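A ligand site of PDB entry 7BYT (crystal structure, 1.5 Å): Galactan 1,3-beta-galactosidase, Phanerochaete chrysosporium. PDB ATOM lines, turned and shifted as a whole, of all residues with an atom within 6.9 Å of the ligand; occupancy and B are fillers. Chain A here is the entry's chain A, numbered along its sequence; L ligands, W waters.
The side-chain carboxylate (OD2) of Asp 137 sits at hydrogen-bond distance from an oxygen (O2) of the ligand (2.6 Å).
The side-chain carboxylate of Glu 81 is in hydrogen-bond range of an oxygen (O4) of the ligand.
O2 of the ligand lies within hydrogen-bond range of NH2 of Arg 82, 2.9 Å away.
OE1 of Gln 242 sits at hydrogen-bond distance from O1 of the ligand, 3.0 Å away.
O1 of the ligand lies within hydrogen-bond range of O of Gly 207, at 3.0 Å.
OH of Tyr 105 sits close to O6 of the ligand.
The side-chain carboxylate of Asp 137 lies within hydrogen-bond range of the backbone NH of Ala 188 (2.8 Å).
OE2 of Glu 81 is in hydrogen-bond range of OH of Tyr 105 (2.6 Å).
O of Glu 81 sits at hydrogen-bond distance from N of His 99, 2.9 Å away.
O of Asn 243 lies within hydrogen-bond range of NH1 of Arg 82, at 3.0 Å.
NE2 of Gln 242 lies within hydrogen-bond range of OE2 of Glu 187.
OE1 of Gln 242 sits at hydrogen-bond distance from NE1 of Trp 260 (2.9 Å).
O of Tyr 105 is in hydrogen-bond range of NH2 of Arg 136.
The backbone NH of Glu 187 sits at hydrogen-bond distance from the backbone carbonyl oxygen of Ser 203 (2.8 Å).
Glu 187 touches the ligand (OE2 to C1, 3.5 Å).
CE2 of Trp 208 touches C6 of the ligand (3.4 Å).
NE1 of Trp 260 touches O1 of the ligand, 3.9 Å away.
Nine residues have an atom within 4 Å of the ligand: Glu 81, Arg 82, Tyr 105, Asp 137, Glu 187, Gly 207, Trp 208, Gln 242 and Trp 260.
The nearest printed residue that does not touch the ligand is Ala 188 (4.6 Å).
Water W2 lies within hydrogen-bond range of OE2 of Glu 36 (2.7 Å) and O3 of the ligand (2.7 Å).
Water W1 lies within hydrogen-bond range of OD1 of Asp 137 and O4 of the ligand.
Water W3 lies within hydrogen-bond range of a ring nitrogen (ND1) of His 99, the side-chain carboxylate of Asp 137, the side-chain carboxylate of Glu 81 and an oxygen (O3) of the ligand.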
ATOM      1  N   GLY A  21      24.894  32.479  22.442  1.00  0.00           N
ATOM      2  CA  GLY A  21      23.435  32.484  22.520  1.00  0.00           C
ATOM      3  C   GLY A  21      22.876  33.724  23.194  1.00  0.00           C
ATOM      4  O   GLY A  21      21.911  33.636  23.973  1.00  0.00           O
ATOM      5  N   GLU A  36      25.742  31.797  27.271  1.00  0.00           N
ATOM      6  CA  GLU A  36      26.256  30.488  27.679  1.00  0.00           C
ATOM      7  C   GLU A  36      27.764  30.541  27.865  1.00  0.00           C
ATOM      8  O   GLU A  36      28.500  30.981  26.971  1.00  0.00           O
ATOM      9  CB  GLU A  36      25.966  29.470  26.570  1.00  0.00           C
ATOM     10  CG  GLU A  36      24.524  29.499  26.079  1.00  0.00           C
ATOM     11  CD  GLU A  36      24.364  28.998  24.649  1.00  0.00           C
ATOM     12  OE1 GLU A  36      25.365  28.519  24.060  1.00  0.00           O
ATOM     13  OE2 GLU A  36      23.236  29.101  24.118  1.00  0.00           O
ATOM     14  N   ALA A  43      28.858  21.512  25.190  1.00  0.00           N
ATOM     15  CA  ALA A  43      27.478  21.960  25.103  1.00  0.00           C
ATOM     16  C   ALA A  43      26.721  21.808  26.415  1.00  0.00           C
ATOM     17  O   ALA A  43      25.613  22.332  26.533  1.00  0.00           O
ATOM     18  CB  ALA A  43      26.746  21.185  24.007  1.00  0.00           C
ATOM     19  N   VAL A  79      21.598  20.702  29.504  1.00  0.00           N
ATOM     20  CA  VAL A  79      21.878  21.767  28.540  1.00  0.00           C
ATOM     21  C   VAL A  79      21.059  22.990  28.914  1.00  0.00           C
ATOM     22  O   VAL A  79      19.855  22.882  29.178  1.00  0.00           O
ATOM     23  CB  VAL A  79      21.534  21.294  27.110  1.00  0.00           C
ATOM     24  CG1 VAL A  79      21.562  22.468  26.123  1.00  0.00           C
ATOM     25  CG2 VAL A  79      22.490  20.201  26.666  1.00  0.00           C
ATOM     26  N   GLU A  81      20.620  26.774  27.133  1.00  0.00           N
ATOM     27  CA  GLU A  81      20.981  27.530  25.949  1.00  0.00           C
ATOM     28  C   GLU A  81      20.139  28.787  25.790  1.00  0.00           C
ATOM     29  O   GLU A  81      18.998  28.863  26.265  1.00  0.00           O
ATOM     30  CB  GLU A  81      20.841  26.668  24.673  1.00  0.00           C
ATOM     31  CG  GLU A  81      22.000  25.694  24.508  1.00  0.00           C
ATOM     32  CD  GLU A  81      21.821  24.699  23.384  1.00  0.00           C
ATOM     33  OE1 GLU A  81      20.785  24.716  22.693  1.00  0.00           O
ATOM     34  OE2 GLU A  81      22.750  23.874  23.180  1.00  0.00           O
ATOM     35  N   ARG A  82      20.723  29.776  25.138  1.00  0.00           N
ATOM     36  CA  ARG A  82      20.007  30.963  24.692  1.00  0.00           C
ATOM     37  C   ARG A  82      19.245  31.697  25.801  1.00  0.00           C
ATOM     38  O   ARG A  82      18.039  31.938  25.688  1.00  0.00           O
ATOM     39  CB  ARG A  82      19.096  30.623  23.511  1.00  0.00           C
ATOM     40  CG  ARG A  82      19.926  30.117  22.306  1.00  0.00           C
ATOM     41  CD  ARG A  82      19.085  29.827  21.066  1.00  0.00           C
ATOM     42  NE  ARG A  82      19.925  29.350  19.972  1.00  0.00           N
ATOM     43  CZ  ARG A  82      20.601  30.160  19.146  1.00  0.00           C
ATOM     44  NH1 ARG A  82      20.515  31.478  19.290  1.00  0.00           N
ATOM     45  NH2 ARG A  82      21.353  29.652  18.179  1.00  0.00           N
ATOM     46  N   HIS A  99      16.415  27.851  27.049  1.00  0.00           N
ATOM     47  CA  HIS A  99      16.151  26.514  26.543  1.00  0.00           C
ATOM     48  C   HIS A  99      16.777  25.532  27.518  1.00  0.00           C
ATOM     49  O   HIS A  99      17.987  25.579  27.767  1.00  0.00           O
ATOM     50  CB  HIS A  99      16.750  26.409  25.149  1.00  0.00           C
ATOM     51  CG  HIS A  99      16.773  25.025  24.573  1.00  0.00           C
ATOM     52  ND1 HIS A  99      17.453  24.731  23.405  1.00  0.00           N
ATOM     53  CD2 HIS A  99      16.168  23.869  24.961  1.00  0.00           C
ATOM     54  CE1 HIS A  99      17.309  23.445  23.125  1.00  0.00           C
ATOM     55  NE2 HIS A  99      16.526  22.902  24.047  1.00  0.00           N
ATOM     56  N   TYR A 105      19.061  16.604  23.448  1.00  0.00           N
ATOM     57  CA  TYR A 105      17.956  17.487  23.064  1.00  0.00           C
ATOM     58  C   TYR A 105      16.616  16.761  23.007  1.00  0.00           C
ATOM     59  O   TYR A 105      15.711  17.165  22.272  1.00  0.00           O
ATOM     60  CB  TYR A 105      18.250  18.268  21.770  1.00  0.00           C
ATOM     61  CG  TYR A 105      19.497  19.124  21.882  1.00  0.00           C
ATOM     62  CD1 TYR A 105      19.434  20.417  22.372  1.00  0.00           C
ATOM     63  CD2 TYR A 105      20.730  18.623  21.491  1.00  0.00           C
ATOM     64  CE1 TYR A 105      20.572  21.207  22.473  1.00  0.00           C
ATOM     65  CE2 TYR A 105      21.880  19.404  21.590  1.00  0.00           C
ATOM     66  CZ  TYR A 105      21.785  20.694  22.083  1.00  0.00           C
ATOM     67  OH  TYR A 105      22.925  21.474  22.186  1.00  0.00           O
ATOM     68  N   ARG A 136      12.556  24.137  21.946  1.00  0.00           N
ATOM     69  CA  ARG A 136      14.012  24.052  21.874  1.00  0.00           C
ATOM     70  C   ARG A 136      14.581  25.460  21.754  1.00  0.00           C
ATOM     71  O   ARG A 136      14.529  26.209  22.724  1.00  0.00           O
ATOM     72  CB  ARG A 136      14.473  23.053  20.807  1.00  0.00           C
ATOM     73  CG  ARG A 136      14.171  21.604  21.235  1.00  0.00           C
ATOM     74  CD  ARG A 136      14.576  20.570  20.186  1.00  0.00           C
ATOM     75  NE  ARG A 136      14.391  19.196  20.673  1.00  0.00           N
ATOM     76  CZ  ARG A 136      13.236  18.542  20.605  1.00  0.00           C
ATOM     77  NH1 ARG A 136      12.162  19.134  20.094  1.00  0.00           N
ATOM     78  NH2 ARG A 136      13.150  17.298  21.060  1.00  0.00           N
ATOM     79  N   ASP A 137      15.115  25.863  20.597  1.00  0.00           N
ATOM     80  CA  ASP A 137      15.535  27.264  20.482  1.00  0.00           C
ATOM     81  C   ASP A 137      14.377  28.174  20.824  1.00  0.00           C
ATOM     82  O   ASP A 137      13.236  27.945  20.400  1.00  0.00           O
ATOM     83  CB  ASP A 137      15.962  27.580  19.046  1.00  0.00           C
ATOM     84  CG  ASP A 137      17.355  27.132  18.736  1.00  0.00           C
ATOM     85  OD1 ASP A 137      17.917  26.287  19.467  1.00  0.00           O
ATOM     86  OD2 ASP A 137      17.881  27.595  17.701  1.00  0.00           O
ATOM     87  N   GLU A 187      14.550  28.225  13.724  1.00  0.00           N
ATOM     88  CA  GLU A 187      15.103  28.273  15.073  1.00  0.00           C
ATOM     89  C   GLU A 187      15.831  29.606  15.255  1.00  0.00           C
ATOM     90  O   GLU A 187      15.660  30.540  14.462  1.00  0.00           O
ATOM     91  CB  GLU A 187      15.867  27.001  15.463  1.00  0.00           C
ATOM     92  CG  GLU A 187      17.056  26.709  14.620  1.00  0.00           C
ATOM     93  CD  GLU A 187      17.873  25.474  15.069  1.00  0.00           C
ATOM     94  OE1 GLU A 187      17.463  24.653  15.936  1.00  0.00           O
ATOM     95  OE2 GLU A 187      18.966  25.329  14.518  1.00  0.00           O
ATOM     96  N   ALA A 188      16.560  29.727  16.356  1.00  0.00           N
ATOM     97  CA  ALA A 188      17.295  30.948  16.723  1.00  0.00           C
ATOM     98  C   ALA A 188      16.462  32.229  16.511  1.00  0.00           C
ATOM     99  O   ALA A 188      16.928  33.161  15.852  1.00  0.00           O
ATOM    100  CB  ALA A 188      18.610  31.020  15.952  1.00  0.00           C
ATOM    101  N   SER A 203      16.773  31.612  11.978  1.00  0.00           N
ATOM    102  CA  SER A 203      17.505  30.715  11.089  1.00  0.00           C
ATOM    103  C   SER A 203      16.621  29.529  10.729  1.00  0.00           C
ATOM    104  O   SER A 203      15.567  29.298  11.321  1.00  0.00           O
ATOM    105  CB  SER A 203      18.786  30.214  11.752  1.00  0.00           C
ATOM    106  OG  SER A 203      18.516  29.202  12.723  1.00  0.00           O
ATOM    107  N   HIS A 204      17.063  28.784   9.736  1.00  0.00           N
ATOM    108  CA  HIS A 204      16.513  27.450   9.539  1.00  0.00           C
ATOM    109  C   HIS A 204      17.289  26.459  10.402  1.00  0.00           C
ATOM    110  O   HIS A 204      18.116  26.844  11.223  1.00  0.00           O
ATOM    111  CB  HIS A 204      16.386  27.107   8.052  1.00  0.00           C
ATOM    112  CG  HIS A 204      15.163  27.670   7.408  1.00  0.00           C
ATOM    113  ND1 HIS A 204      13.891  27.196   7.665  1.00  0.00           N
ATOM    114  CD2 HIS A 204      15.013  28.694   6.522  1.00  0.00           C
ATOM    115  CE1 HIS A 204      13.022  27.893   6.954  1.00  0.00           C
ATOM    116  NE2 HIS A 204      13.670  28.802   6.261  1.00  0.00           N
ATOM    117  N   SER A 206      19.860  23.654  10.707  1.00  0.00           N
ATOM    118  CA  SER A 206      21.005  22.909  10.194  1.00  0.00           C
ATOM    119  C   SER A 206      22.012  22.608  11.306  1.00  0.00           C
ATOM    120  O   SER A 206      23.225  22.609  11.071  1.00  0.00           O
ATOM    121  CB  SER A 206      21.656  23.606   8.996  1.00  0.00           C
ATOM    122  OG  SER A 206      22.038  24.948   9.313  1.00  0.00           O
ATOM    123  N   GLY A 207      21.523  22.372  12.519  1.00  0.00           N
ATOM    124  CA  GLY A 207      22.450  22.101  13.623  1.00  0.00           C
ATOM    125  C   GLY A 207      23.368  23.281  13.851  1.00  0.00           C
ATOM    126  O   GLY A 207      22.963  24.442  13.770  1.00  0.00           O
ATOM    127  N   TRP A 208      24.645  22.984  14.134  1.00  0.00           N
ATOM    128  CA  TRP A 208      25.609  24.050  14.378  1.00  0.00           C
ATOM    129  C   TRP A 208      26.042  24.769  13.097  1.00  0.00           C
ATOM    130  O   TRP A 208      26.659  25.831  13.205  1.00  0.00           O
ATOM    131  CB  TRP A 208      26.868  23.498  15.059  1.00  0.00           C
ATOM    132  CG  TRP A 208      26.714  22.880  16.429  1.00  0.00           C
ATOM    133  CD1 TRP A 208      26.825  21.557  16.747  1.00  0.00           C
ATOM    134  CD2 TRP A 208      26.464  23.566  17.676  1.00  0.00           C
ATOM    135  NE1 TRP A 208      26.649  21.372  18.101  1.00  0.00           N
ATOM    136  CE2 TRP A 208      26.434  22.590  18.687  1.00  0.00           C
ATOM    137  CE3 TRP A 208      26.265  24.902  18.024  1.00  0.00           C
ATOM    138  CZ2 TRP A 208      26.204  22.908  20.036  1.00  0.00           C
ATOM    139  CZ3 TRP A 208      26.027  25.216  19.354  1.00  0.00           C
ATOM    140  CH2 TRP A 208      25.998  24.225  20.336  1.00  0.00           C
ATOM    141  N   ALA A 209      25.747  24.229  11.913  1.00  0.00           N
ATOM    142  CA  ALA A 209      26.193  24.864  10.678  1.00  0.00           C
ATOM    143  C   ALA A 209      25.346  26.097  10.372  1.00  0.00           C
ATOM    144  O   ALA A 209      24.128  26.083  10.589  1.00  0.00           O
ATOM    145  CB  ALA A 209      26.079  23.888   9.502  1.00  0.00           C
ATOM    146  N   GLN A 242      24.699  32.673  13.116  1.00  0.00           N
ATOM    147  CA  GLN A 242      23.319  32.304  13.415  1.00  0.00           C
ATOM    148  C   GLN A 242      22.768  33.319  14.395  1.00  0.00           C
ATOM    149  O   GLN A 242      23.444  33.669  15.370  1.00  0.00           O
ATOM    150  CB  GLN A 242      23.256  30.902  14.014  1.00  0.00           C
ATOM    151  CG  GLN A 242      21.825  30.430  14.279  1.00  0.00           C
ATOM    152  CD  GLN A 242      21.759  29.065  14.926  1.00  0.00           C
ATOM    153  OE1 GLN A 242      22.667  28.663  15.670  1.00  0.00           O
ATOM    154  NE2 GLN A 242      20.662  28.349  14.673  1.00  0.00           N
ATOM    155  N   ASN A 243      21.561  33.773  14.150  1.00  0.00           N
ATOM    156  CA  ASN A 243      20.907  34.786  15.007  1.00  0.00           C
ATOM    157  C   ASN A 243      20.991  34.395  16.465  1.00  0.00           C
ATOM    158  O   ASN A 243      20.813  33.214  16.812  1.00  0.00           O
ATOM    159  CB  ASN A 243      19.452  34.920  14.608  1.00  0.00           C
ATOM    160  CG  ASN A 243      18.809  36.167  15.127  1.00  0.00           C
ATOM    161  OD1 ASN A 243      19.394  37.252  15.079  1.00  0.00           O
ATOM    162  ND2 ASN A 243      17.576  36.033  15.638  1.00  0.00           N
ATOM    163  N   TRP A 260      29.352  29.565  15.479  1.00  0.00           N
ATOM    164  CA  TRP A 260      29.604  28.375  16.272  1.00  0.00           C
ATOM    165  C   TRP A 260      30.795  27.608  15.712  1.00  0.00           C
ATOM    166  O   TRP A 260      30.933  27.434  14.502  1.00  0.00           O
ATOM    167  CB  TRP A 260      28.378  27.461  16.230  1.00  0.00           C
ATOM    168  CG  TRP A 260      27.164  28.044  16.869  1.00  0.00           C
ATOM    169  CD1 TRP A 260      26.002  28.391  16.236  1.00  0.00           C
ATOM    170  CD2 TRP A 260      26.975  28.333  18.262  1.00  0.00           C
ATOM    171  NE1 TRP A 260      25.097  28.882  17.145  1.00  0.00           N
ATOM    172  CE2 TRP A 260      25.669  28.844  18.394  1.00  0.00           C
ATOM    173  CE3 TRP A 260      27.781  28.196  19.407  1.00  0.00           C
ATOM    174  CZ2 TRP A 260      25.149  29.229  19.623  1.00  0.00           C
ATOM    175  CZ3 TRP A 260      27.250  28.568  20.632  1.00  0.00           C
ATOM    176  CH2 TRP A 260      25.940  29.094  20.730  1.00  0.00           C
HETATM  177  C1  LIG L   1      21.573  25.073  16.787  1.00  0.00           C
HETATM  178  C2  LIG L   1      20.843  25.794  17.919  1.00  0.00           C
HETATM  179  C3  LIG L   1      21.788  25.914  19.099  1.00  0.00           C
HETATM  180  C4  LIG L   1      22.174  24.508  19.577  1.00  0.00           C
HETATM  181  C5  LIG L   1      22.768  23.721  18.392  1.00  0.00           C
HETATM  182  C6  LIG L   1      23.035  22.260  18.753  1.00  0.00           C
HETATM  183  O1  LIG L   1      22.762  25.809  16.442  1.00  0.00           O
HETATM  184  O2  LIG L   1      20.427  27.062  17.426  1.00  0.00           O
HETATM  185  O3  LIG L   1      21.194  26.663  20.172  1.00  0.00           O
HETATM  186  O4  LIG L   1      21.058  23.808  20.159  1.00  0.00           O
HETATM  187  O5  LIG L   1      21.903  23.759  17.246  1.00  0.00           O
HETATM  188  O6  LIG L   1      21.811  21.537  18.879  1.00  0.00           O
HETATM  189  O   HOH W   1      18.249  23.525  19.929  1.00  0.00           O
HETATM  190  O   HOH W   2      23.126  27.598  21.858  1.00  0.00           O
HETATM  191  O   HOH W   3      18.798  26.539  21.978  1.00  0.00           O
HETATM  192  O   HOH W   4      22.219  19.013  18.016  1.00  0.00           O
